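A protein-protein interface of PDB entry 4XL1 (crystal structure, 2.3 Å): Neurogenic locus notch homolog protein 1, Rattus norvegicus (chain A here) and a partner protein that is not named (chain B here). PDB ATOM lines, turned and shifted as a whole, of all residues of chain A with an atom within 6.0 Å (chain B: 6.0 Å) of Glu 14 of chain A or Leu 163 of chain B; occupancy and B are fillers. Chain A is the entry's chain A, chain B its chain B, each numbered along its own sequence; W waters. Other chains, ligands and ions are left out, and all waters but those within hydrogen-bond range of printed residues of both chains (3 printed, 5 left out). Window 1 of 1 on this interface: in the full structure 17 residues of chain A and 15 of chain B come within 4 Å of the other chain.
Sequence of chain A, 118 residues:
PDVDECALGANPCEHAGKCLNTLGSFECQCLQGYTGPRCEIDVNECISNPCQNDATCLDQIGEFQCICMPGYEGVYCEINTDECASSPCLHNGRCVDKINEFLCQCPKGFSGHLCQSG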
ATOM      1  N   ASN A  11     -26.532 -19.408  -8.130  1.00  0.00           N
ATOM      2  CA  ASN A  11     -25.348 -20.240  -7.922  1.00  0.00           C
ATOM      3  C   ASN A  11     -25.425 -20.980  -6.593  1.00  0.00           C
ATOM      4  O   ASN A  11     -25.483 -20.362  -5.532  1.00  0.00           O
ATOM      5  CB  ASN A  11     -24.087 -19.364  -7.955  1.00  0.00           C
ATOM      6  CG  ASN A  11     -22.791 -20.164  -7.882  1.00  0.00           C
ATOM      7  OD1 ASN A  11     -22.793 -21.372  -7.647  1.00  0.00           O
ATOM      8  ND2 ASN A  11     -21.668 -19.474  -8.047  1.00  0.00           N
ATOM      9  N   PRO A  12     -25.436 -22.322  -6.662  1.00  0.00           N
ATOM     10  CA  PRO A  12     -25.537 -23.192  -5.485  1.00  0.00           C
ATOM     11  C   PRO A  12     -24.226 -23.312  -4.726  1.00  0.00           C
ATOM     12  O   PRO A  12     -24.201 -23.877  -3.635  1.00  0.00           O
ATOM     13  CB  PRO A  12     -25.937 -24.545  -6.075  1.00  0.00           C
ATOM     14  CG  PRO A  12     -25.487 -24.509  -7.489  1.00  0.00           C
ATOM     15  CD  PRO A  12     -25.352 -23.084  -7.921  1.00  0.00           C
ATOM     16  N   CYS A  13     -23.152 -22.773  -5.289  1.00  0.00           N
ATOM     17  CA  CYS A  13     -21.844 -22.887  -4.664  1.00  0.00           C
ATOM     18  C   CYS A  13     -21.548 -21.635  -3.856  1.00  0.00           C
ATOM     19  O   CYS A  13     -21.478 -20.539  -4.407  1.00  0.00           O
ATOM     20  CB  CYS A  13     -20.758 -23.107  -5.717  1.00  0.00           C
ATOM     21  SG  CYS A  13     -21.031 -24.540  -6.789  1.00  0.00           S
ATOM     22  N   GLU A  14     -21.377 -21.793  -2.550  1.00  0.00           N
ATOM     23  CA  GLU A  14     -21.122 -20.645  -1.692  1.00  0.00           C
ATOM     24  C   GLU A  14     -19.692 -20.133  -1.865  1.00  0.00           C
ATOM     25  O   GLU A  14     -18.859 -20.808  -2.470  1.00  0.00           O
ATOM     26  CB  GLU A  14     -21.382 -21.012  -0.227  1.00  0.00           C
ATOM     27  CG  GLU A  14     -22.741 -21.656   0.025  1.00  0.00           C
ATOM     28  CD  GLU A  14     -23.876 -20.647   0.056  1.00  0.00           C
ATOM     29  OE1 GLU A  14     -23.612 -19.444  -0.157  1.00  0.00           O
ATOM     30  OE2 GLU A  14     -25.033 -21.052   0.299  1.00  0.00           O
ATOM     31  N   HIS A  15     -19.415 -18.951  -1.323  1.00  0.00           N
ATOM     32  CA  HIS A  15     -18.093 -18.329  -1.400  1.00  0.00           C
ATOM     33  C   HIS A  15     -17.532 -18.256  -2.827  1.00  0.00           C
ATOM     34  O   HIS A  15     -16.368 -18.605  -3.059  1.00  0.00           O
ATOM     35  CB  HIS A  15     -17.090 -19.088  -0.545  1.00  0.00           C
ATOM     36  CG  HIS A  15     -17.410 -19.124   0.917  1.00  0.00           C
ATOM     37  ND1 HIS A  15     -17.724 -20.281   1.596  1.00  0.00           N
ATOM     38  CD2 HIS A  15     -17.487 -18.124   1.824  1.00  0.00           C
ATOM     39  CE1 HIS A  15     -17.970 -19.992   2.861  1.00  0.00           C
ATOM     40  NE2 HIS A  15     -17.833 -18.689   3.027  1.00  0.00           N
ATOM     41  N   ALA A  16     -18.377 -17.795  -3.753  1.00  0.00           N
ATOM     42  CA  ALA A  16     -17.981 -17.623  -5.158  1.00  0.00           C
ATOM     43  C   ALA A  16     -17.420 -18.895  -5.803  1.00  0.00           C
ATOM     44  O   ALA A  16     -16.525 -18.820  -6.648  1.00  0.00           O
ATOM     45  CB  ALA A  16     -16.969 -16.489  -5.287  1.00  0.00           C
ATOM     46  N   GLY A  17     -17.950 -20.049  -5.413  1.00  0.00           N
ATOM     47  CA  GLY A  17     -17.556 -21.315  -6.013  1.00  0.00           C
ATOM     48  C   GLY A  17     -18.048 -21.469  -7.441  1.00  0.00           C
ATOM     49  O   GLY A  17     -18.911 -20.713  -7.881  1.00  0.00           O
ATOM     50  N   CYS A  28     -19.670 -28.641  -7.327  1.00  0.00           N
ATOM     51  CA  CYS A  28     -19.044 -27.330  -7.123  1.00  0.00           C
ATOM     52  C   CYS A  28     -17.518 -27.404  -7.168  1.00  0.00           C
ATOM     53  O   CYS A  28     -16.904 -28.267  -6.536  1.00  0.00           O
ATOM     54  CB  CYS A  28     -19.475 -26.721  -5.784  1.00  0.00           C
ATOM     55  SG  CYS A  28     -21.206 -26.234  -5.685  1.00  0.00           S
ATOM     56  N   CYS A  30     -14.711 -25.397  -5.736  1.00  0.00           N
ATOM     57  CA  CYS A  30     -14.604 -24.389  -4.693  1.00  0.00           C
ATOM     58  C   CYS A  30     -13.299 -23.613  -4.806  1.00  0.00           C
ATOM     59  O   CYS A  30     -12.273 -24.170  -5.196  1.00  0.00           O
ATOM     60  CB  CYS A  30     -14.706 -25.047  -3.315  1.00  0.00           C
ATOM     61  SG  CYS A  30     -16.274 -25.897  -3.001  1.00  0.00           S
ATOM     62  N   TYR A  34     -11.929 -23.606   0.761  1.00  0.00           N
ATOM     63  CA  TYR A  34     -13.303 -24.004   1.043  1.00  0.00           C
ATOM     64  C   TYR A  34     -13.588 -25.433   0.594  1.00  0.00           C
ATOM     65  O   TYR A  34     -13.076 -25.894  -0.425  1.00  0.00           O
ATOM     66  CB  TYR A  34     -14.284 -23.034   0.383  1.00  0.00           C
ATOM     67  CG  TYR A  34     -14.180 -21.631   0.933  1.00  0.00           C
ATOM     68  CD1 TYR A  34     -14.628 -21.336   2.214  1.00  0.00           C
ATOM     69  CD2 TYR A  34     -13.632 -20.605   0.177  1.00  0.00           C
ATOM     70  CE1 TYR A  34     -14.531 -20.058   2.727  1.00  0.00           C
ATOM     71  CE2 TYR A  34     -13.534 -19.322   0.681  1.00  0.00           C
ATOM     72  CZ  TYR A  34     -13.985 -19.054   1.956  1.00  0.00           C
ATOM     73  OH  TYR A  34     -13.887 -17.777   2.458  1.00  0.00           O
ATOM     74  N   ARG A  38     -21.211 -27.797  -1.358  1.00  0.00           N
ATOM     75  CA  ARG A  38     -21.578 -26.482  -1.863  1.00  0.00           C
ATOM     76  C   ARG A  38     -20.681 -25.389  -1.283  1.00  0.00           C
ATOM     77  O   ARG A  38     -21.096 -24.236  -1.148  1.00  0.00           O
ATOM     78  CB  ARG A  38     -23.054 -26.199  -1.569  1.00  0.00           C
ATOM     79  CG  ARG A  38     -23.973 -27.285  -2.114  1.00  0.00           C
ATOM     80  CD  ARG A  38     -25.412 -26.823  -2.266  1.00  0.00           C
ATOM     81  NE  ARG A  38     -26.252 -27.896  -2.790  1.00  0.00           N
ATOM     82  CZ  ARG A  38     -27.563 -27.796  -2.985  1.00  0.00           C
ATOM     83  NH1 ARG A  38     -28.196 -26.667  -2.701  1.00  0.00           N
ATOM     84  NH2 ARG A  38     -28.243 -28.828  -3.468  1.00  0.00           N
ATOM     85  N   CYS A  39     -19.463 -25.784  -0.921  1.00  0.00           N
ATOM     86  CA  CYS A  39     -18.393 -24.861  -0.537  1.00  0.00           C
ATOM     87  C   CYS A  39     -18.691 -24.076   0.737  1.00  0.00           C
ATOM     88  O   CYS A  39     -18.119 -23.008   0.950  1.00  0.00           O
ATOM     89  CB  CYS A  39     -18.114 -23.874  -1.676  1.00  0.00           C
ATOM     90  SG  CYS A  39     -17.826 -24.623  -3.293  1.00  0.00           S
ATOM     91  N   GLU A  40     -19.568 -24.598   1.590  1.00  0.00           N
ATOM     92  CA  GLU A  40     -20.009 -23.837   2.758  1.00  0.00           C
ATOM     93  C   GLU A  40     -19.076 -23.962   3.965  1.00  0.00           C
ATOM     94  O   GLU A  40     -19.277 -23.288   4.975  1.00  0.00           O
ATOM     95  CB  GLU A  40     -21.426 -24.257   3.170  1.00  0.00           C
ATOM     96  CG  GLU A  40     -21.544 -25.657   3.761  1.00  0.00           C
ATOM     97  CD  GLU A  40     -21.800 -26.726   2.716  1.00  0.00           C
ATOM     98  OE1 GLU A  40     -21.172 -26.677   1.637  1.00  0.00           O
ATOM     99  OE2 GLU A  40     -22.639 -27.616   2.974  1.00  0.00           O
ATOM    100  N   ILE A  41     -18.065 -24.820   3.865  1.00  0.00           N
ATOM    101  CA  ILE A  41     -17.172 -25.074   4.995  1.00  0.00           C
ATOM    102  C   ILE A  41     -15.770 -24.494   4.813  1.00  0.00           C
ATOM    103  O   ILE A  41     -15.099 -24.745   3.809  1.00  0.00           O
ATOM    104  CB  ILE A  41     -17.051 -26.582   5.288  1.00  0.00           C
ATOM    105  CG1 ILE A  41     -18.423 -27.159   5.632  1.00  0.00           C
ATOM    106  CG2 ILE A  41     -16.102 -26.825   6.453  1.00  0.00           C
ATOM    107  CD1 ILE A  41     -19.031 -26.569   6.894  1.00  0.00           C
ATOM    108  N   ASN B 154     -24.818 -14.936   8.680  1.00  0.00           N
ATOM    109  CA  ASN B 154     -24.786 -16.173   7.870  1.00  0.00           C
ATOM    110  C   ASN B 154     -23.648 -17.167   8.213  1.00  0.00           C
ATOM    111  O   ASN B 154     -23.493 -18.172   7.511  1.00  0.00           O
ATOM    112  CB  ASN B 154     -24.688 -15.870   6.360  1.00  0.00           C
ATOM    113  CG  ASN B 154     -25.740 -14.904   5.865  1.00  0.00           C
ATOM    114  OD1 ASN B 154     -25.406 -13.941   5.172  1.00  0.00           O
ATOM    115  ND2 ASN B 154     -27.001 -15.145   6.204  1.00  0.00           N
ATOM    116  N   TYR B 155     -22.859 -16.913   9.262  1.00  0.00           N
ATOM    117  CA  TYR B 155     -21.880 -17.916   9.708  1.00  0.00           C
ATOM    118  C   TYR B 155     -22.391 -18.556  10.990  1.00  0.00           C
ATOM    119  O   TYR B 155     -23.026 -17.894  11.816  1.00  0.00           O
ATOM    120  CB  TYR B 155     -20.469 -17.328   9.919  1.00  0.00           C
ATOM    121  CG  TYR B 155     -19.822 -16.898   8.616  1.00  0.00           C
ATOM    122  CD1 TYR B 155     -19.337 -17.844   7.717  1.00  0.00           C
ATOM    123  CD2 TYR B 155     -19.614 -15.555   8.325  1.00  0.00           C
ATOM    124  CE1 TYR B 155     -18.745 -17.461   6.514  1.00  0.00           C
ATOM    125  CE2 TYR B 155     -19.019 -15.161   7.125  1.00  0.00           C
ATOM    126  CZ  TYR B 155     -18.586 -16.117   6.230  1.00  0.00           C
ATOM    127  OH  TYR B 155     -17.990 -15.701   5.057  1.00  0.00           O
ATOM    128  N   TYR B 156     -22.136 -19.851  11.140  1.00  0.00           N
ATOM    129  CA  TYR B 156     -22.667 -20.606  12.265  1.00  0.00           C
ATOM    130  C   TYR B 156     -21.670 -21.639  12.763  1.00  0.00           C
ATOM    131  O   TYR B 156     -20.657 -21.910  12.118  1.00  0.00           O
ATOM    132  CB  TYR B 156     -23.968 -21.325  11.889  1.00  0.00           C
ATOM    133  CG  TYR B 156     -25.089 -20.451  11.376  1.00  0.00           C
ATOM    134  CD1 TYR B 156     -25.140 -20.065  10.044  1.00  0.00           C
ATOM    135  CD2 TYR B 156     -26.113 -20.038  12.218  1.00  0.00           C
ATOM    136  CE1 TYR B 156     -26.165 -19.275   9.567  1.00  0.00           C
ATOM    137  CE2 TYR B 156     -27.146 -19.246  11.751  1.00  0.00           C
ATOM    138  CZ  TYR B 156     -27.166 -18.868  10.424  1.00  0.00           C
ATOM    139  OH  TYR B 156     -28.191 -18.082   9.948  1.00  0.00           O
ATOM    140  N   CYS B 160     -17.627 -20.790  13.982  1.00  0.00           N
ATOM    141  CA  CYS B 160     -18.148 -19.881  12.958  1.00  0.00           C
ATOM    142  C   CYS B 160     -17.664 -20.270  11.565  1.00  0.00           C
ATOM    143  O   CYS B 160     -17.525 -19.417  10.688  1.00  0.00           O
ATOM    144  CB  CYS B 160     -17.757 -18.429  13.257  1.00  0.00           C
ATOM    145  SG  CYS B 160     -18.460 -17.744  14.773  1.00  0.00           S
ATOM    146  N   SER B 161     -17.418 -21.561  11.365  1.00  0.00           N
ATOM    147  CA  SER B 161     -16.809 -22.038  10.130  1.00  0.00           C
ATOM    148  C   SER B 161     -17.831 -22.567   9.128  1.00  0.00           C
ATOM    149  O   SER B 161     -17.469 -22.967   8.023  1.00  0.00           O
ATOM    150  CB  SER B 161     -15.783 -23.132  10.435  1.00  0.00           C
ATOM    151  OG  SER B 161     -14.712 -22.632  11.217  1.00  0.00           O
ATOM    152  N   ARG B 162     -19.106 -22.556   9.500  1.00  0.00           N
ATOM    153  CA  ARG B 162     -20.125 -23.110   8.619  1.00  0.00           C
ATOM    154  C   ARG B 162     -21.093 -22.029   8.152  1.00  0.00           C
ATOM    155  O   ARG B 162     -21.704 -21.332   8.961  1.00  0.00           O
ATOM    156  CB  ARG B 162     -20.881 -24.237   9.323  1.00  0.00           C
ATOM    157  CG  ARG B 162     -22.036 -24.808   8.522  1.00  0.00           C
ATOM    158  CD  ARG B 162     -22.575 -26.073   9.167  1.00  0.00           C
ATOM    159  NE  ARG B 162     -23.465 -26.798   8.268  1.00  0.00           N
ATOM    160  CZ  ARG B 162     -24.091 -27.927   8.582  1.00  0.00           C
ATOM    161  NH1 ARG B 162     -23.930 -28.468   9.782  1.00  0.00           N
ATOM    162  NH2 ARG B 162     -24.883 -28.514   7.696  1.00  0.00           N
ATOM    163  N   LEU B 163     -21.224 -21.902   6.836  1.00  0.00           N
ATOM    164  CA  LEU B 163     -22.057 -20.865   6.241  1.00  0.00           C
ATOM    165  C   LEU B 163     -23.415 -21.418   5.827  1.00  0.00           C
ATOM    166  O   LEU B 163     -23.497 -22.433   5.136  1.00  0.00           O
ATOM    167  CB  LEU B 163     -21.349 -20.236   5.037  1.00  0.00           C
ATOM    168  CG  LEU B 163     -22.050 -19.070   4.334  1.00  0.00           C
ATOM    169  CD1 LEU B 163     -21.049 -17.995   3.951  1.00  0.00           C
ATOM    170  CD2 LEU B 163     -22.790 -19.554   3.100  1.00  0.00           C
ATOM    171  N   CYS B 164     -24.478 -20.750   6.261  1.00  0.00           N
ATOM    172  CA  CYS B 164     -25.823 -21.089   5.814  1.00  0.00           C
ATOM    173  C   CYS B 164     -26.562 -19.851   5.328  1.00  0.00           C
ATOM    174  O   CYS B 164     -26.652 -18.850   6.037  1.00  0.00           O
ATOM    175  CB  CYS B 164     -26.615 -21.764   6.937  1.00  0.00           C
ATOM    176  SG  CYS B 164     -28.343 -22.109   6.519  1.00  0.00           S
ATOM    177  N   MLY B 165     -27.089 -19.924   4.112  1.00  0.00           N
ATOM    178  CA  MLY B 165     -27.909 -18.849   3.572  1.00  0.00           C
ATOM    179  CB  MLY B 165     -27.168 -18.112   2.457  1.00  0.00           C
ATOM    180  CG  MLY B 165     -25.900 -17.414   2.918  1.00  0.00           C
ATOM    181  CD  MLY B 165     -25.154 -16.800   1.749  1.00  0.00           C
ATOM    182  CE  MLY B 165     -25.957 -15.682   1.112  1.00  0.00           C
ATOM    183  NZ  MLY B 165     -25.568 -15.480  -0.310  1.00  0.00           N
ATOM    184  CH1 MLY B 165     -26.784 -15.046  -1.010  1.00  0.00           C
ATOM    185  CH2 MLY B 165     -24.632 -14.351  -0.349  1.00  0.00           C
ATOM    186  C   MLY B 165     -29.213 -19.434   3.055  1.00  0.00           C
ATOM    187  O   MLY B 165     -29.200 -20.351   2.230  1.00  0.00           O
ATOM    188  N   ARG B 167     -32.679 -20.421   1.295  1.00  0.00           N
ATOM    189  CA  ARG B 167     -33.064 -20.533  -0.104  1.00  0.00           C
ATOM    190  C   ARG B 167     -34.527 -20.926  -0.216  1.00  0.00           C
ATOM    191  O   ARG B 167     -35.059 -21.618   0.652  1.00  0.00           O
ATOM    192  CB  ARG B 167     -32.211 -21.576  -0.830  1.00  0.00           C
ATOM    193  CG  ARG B 167     -30.737 -21.253  -0.975  1.00  0.00           C
ATOM    194  CD  ARG B 167     -30.057 -22.299  -1.846  1.00  0.00           C
ATOM    195  NE  ARG B 167     -30.240 -22.028  -3.269  1.00  0.00           N
ATOM    196  CZ  ARG B 167     -29.270 -21.623  -4.082  1.00  0.00           C
ATOM    197  NH1 ARG B 167     -28.039 -21.460  -3.618  1.00  0.00           N
ATOM    198  NH2 ARG B 167     -29.526 -21.395  -5.363  1.00  0.00           N
ATOM    199  N   TYR B 174     -35.189 -23.992   2.484  1.00  0.00           N
ATOM    200  CA  TYR B 174     -34.852 -24.148   3.892  1.00  0.00           C
ATOM    201  C   TYR B 174     -34.586 -22.829   4.604  1.00  0.00           C
ATOM    202  O   TYR B 174     -34.374 -21.792   3.974  1.00  0.00           O
ATOM    203  CB  TYR B 174     -33.634 -25.066   4.039  1.00  0.00           C
ATOM    204  CG  TYR B 174     -32.398 -24.593   3.302  1.00  0.00           C
ATOM    205  CD1 TYR B 174     -31.536 -23.663   3.872  1.00  0.00           C
ATOM    206  CD2 TYR B 174     -32.098 -25.071   2.033  1.00  0.00           C
ATOM    207  CE1 TYR B 174     -30.408 -23.230   3.204  1.00  0.00           C
ATOM    208  CE2 TYR B 174     -30.974 -24.643   1.355  1.00  0.00           C
ATOM    209  CZ  TYR B 174     -30.133 -23.722   1.945  1.00  0.00           C
ATOM    210  OH  TYR B 174     -29.012 -23.293   1.273  1.00  0.00           O
ATOM    211  N   GLY B 180     -26.195 -23.938  11.841  1.00  0.00           N
ATOM    212  CA  GLY B 180     -25.886 -23.717  10.440  1.00  0.00           C
ATOM    213  C   GLY B 180     -26.443 -24.767   9.505  1.00  0.00           C
ATOM    214  O   GLY B 180     -26.283 -24.671   8.288  1.00  0.00           O
HETATM  215  O   HOH W   1     -15.079 -17.041   5.071  1.00  0.00           O
HETATM  216  O   HOH W   2     -27.662 -24.761  -1.085  1.00  0.00           O
HETATM  217  O   HOH W   3     -25.773 -22.601  -1.843  1.00  0.00           O
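The backbone carbonyl oxygen (O) of Asn 11 of chain A is in hydrogen-bond range of the guanidinium group (NH1) of Arg 167 of chain B (3.4 Å).
The backbone carbonyl oxygen (O) of Glu 40 of chain A sits at hydrogen-bond distance from the backbone NH (N) of Leu 163 of chain B, 3.0 Å away.
ND1 of His 15 of chain A lies within hydrogen-bond range of O of Cys 39 of chain A (2.8 Å).
The backbone NH (N) of Ser 161 of chain B is in hydrogen-bond range of the backbone carbonyl oxygen (O) of Tyr 156 of chain B.
The backbone NH of Tyr 156 of chain B lies within hydrogen-bond range of the backbone carbonyl oxygen of Arg 162 of chain B (2.7 Å).
O of Arg 167 of chain B sits at hydrogen-bond distance from N of Tyr 174 of chain B (3.0 Å).
The side-chain sulfur (SG) of Cys 13 of chain A is disulfide-bonded to the side-chain sulfur (SG) of Cys 28 of chain A (2.0 Å).
SG of Cys 39 of chain A is disulfide-bonded to SG of Cys 30 of chain A.
Pro 12 of chain A touches Arg 167 of chain B.
Glu 14 of chain A touches Leu 163 of chain B.
MLY 165 of chain B touches Glu 14 of chain A (CD to OE1, 3.6 Å).
OH of Tyr 155 of chain B touches NE2 of His 15 of chain A (3.6 Å).
His 15 of chain A touches Leu 163 of chain B (NE2 to CD1, 3.4 Å).
Glu 40 of chain A touches Ser 161 of chain B (O to O, 3.6 Å).
Arg 162 of chain B touches Glu 40 of chain A (CA to O, 3.7 Å).
CA of Ile 41 of chain A touches O of Ser 161 of chain B, 3.7 Å away.
CB of Arg 162 of chain B touches CD1 of Ile 41 of chain A, 3.8 Å away.
Glu 14 of chain A touches two residues of chain B.
Of the printed residues of chain A, Leu 163 of chain B touches Glu 14, His 15 and Glu 40.
Of the printed residues of chain B, Pro 12 of chain A touches Arg 167 (3.6 Å).
Printed residues of chain A within 4 Å of Tyr 155 of chain B: His 15.
Of the printed residues of chain B, His 15 of chain A touches Tyr 155 (3.6 Å) and Leu 163 (3.4 Å).
Cys 13 of chain A touches none of the printed residues of chain B.
Cys 39 of chain A touches none of the printed residues of chain B.
The nearest residue of chain A that does not touch Leu 163 of chain B is Ile 41 of chain A (5.2 Å).
Printed residues of chain A that touch a printed residue of chain B: Asn 11, Pro 12, Glu 14, His 15, Glu 40 and Ile 41.
Along chain B the printed residues that touch a printed residue of chain A span positions 155 to 167.
Among the printed residues, 11 pairs touch across the chains.
Among the printed residues, no Asp or Glu carboxylate lies within 4 Å of a Lys or Arg side-chain nitrogen of the other chain.
Water W2 lies within hydrogen-bond range of NH1 of Arg 38 of chain A (2.6 Å) and OH of Tyr 174 of chain B (3.1 Å).
Water W3 lies within hydrogen-bond range of the backbone carbonyl oxygen (O) of Pro 12 of chain A (2.7 Å), the side-chain carboxylate (OE2) of Glu 14 of chain A (2.7 Å) and the guanidinium group (NH1) of Arg 167 of chain B (3.1 Å).
Water W1 lies within hydrogen-bond range of the side-chain hydroxyl (OH) of Tyr 34 of chain A (3.0 Å) and the side-chain hydroxyl (OH) of Tyr 155 of chain B (3.2 Å).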
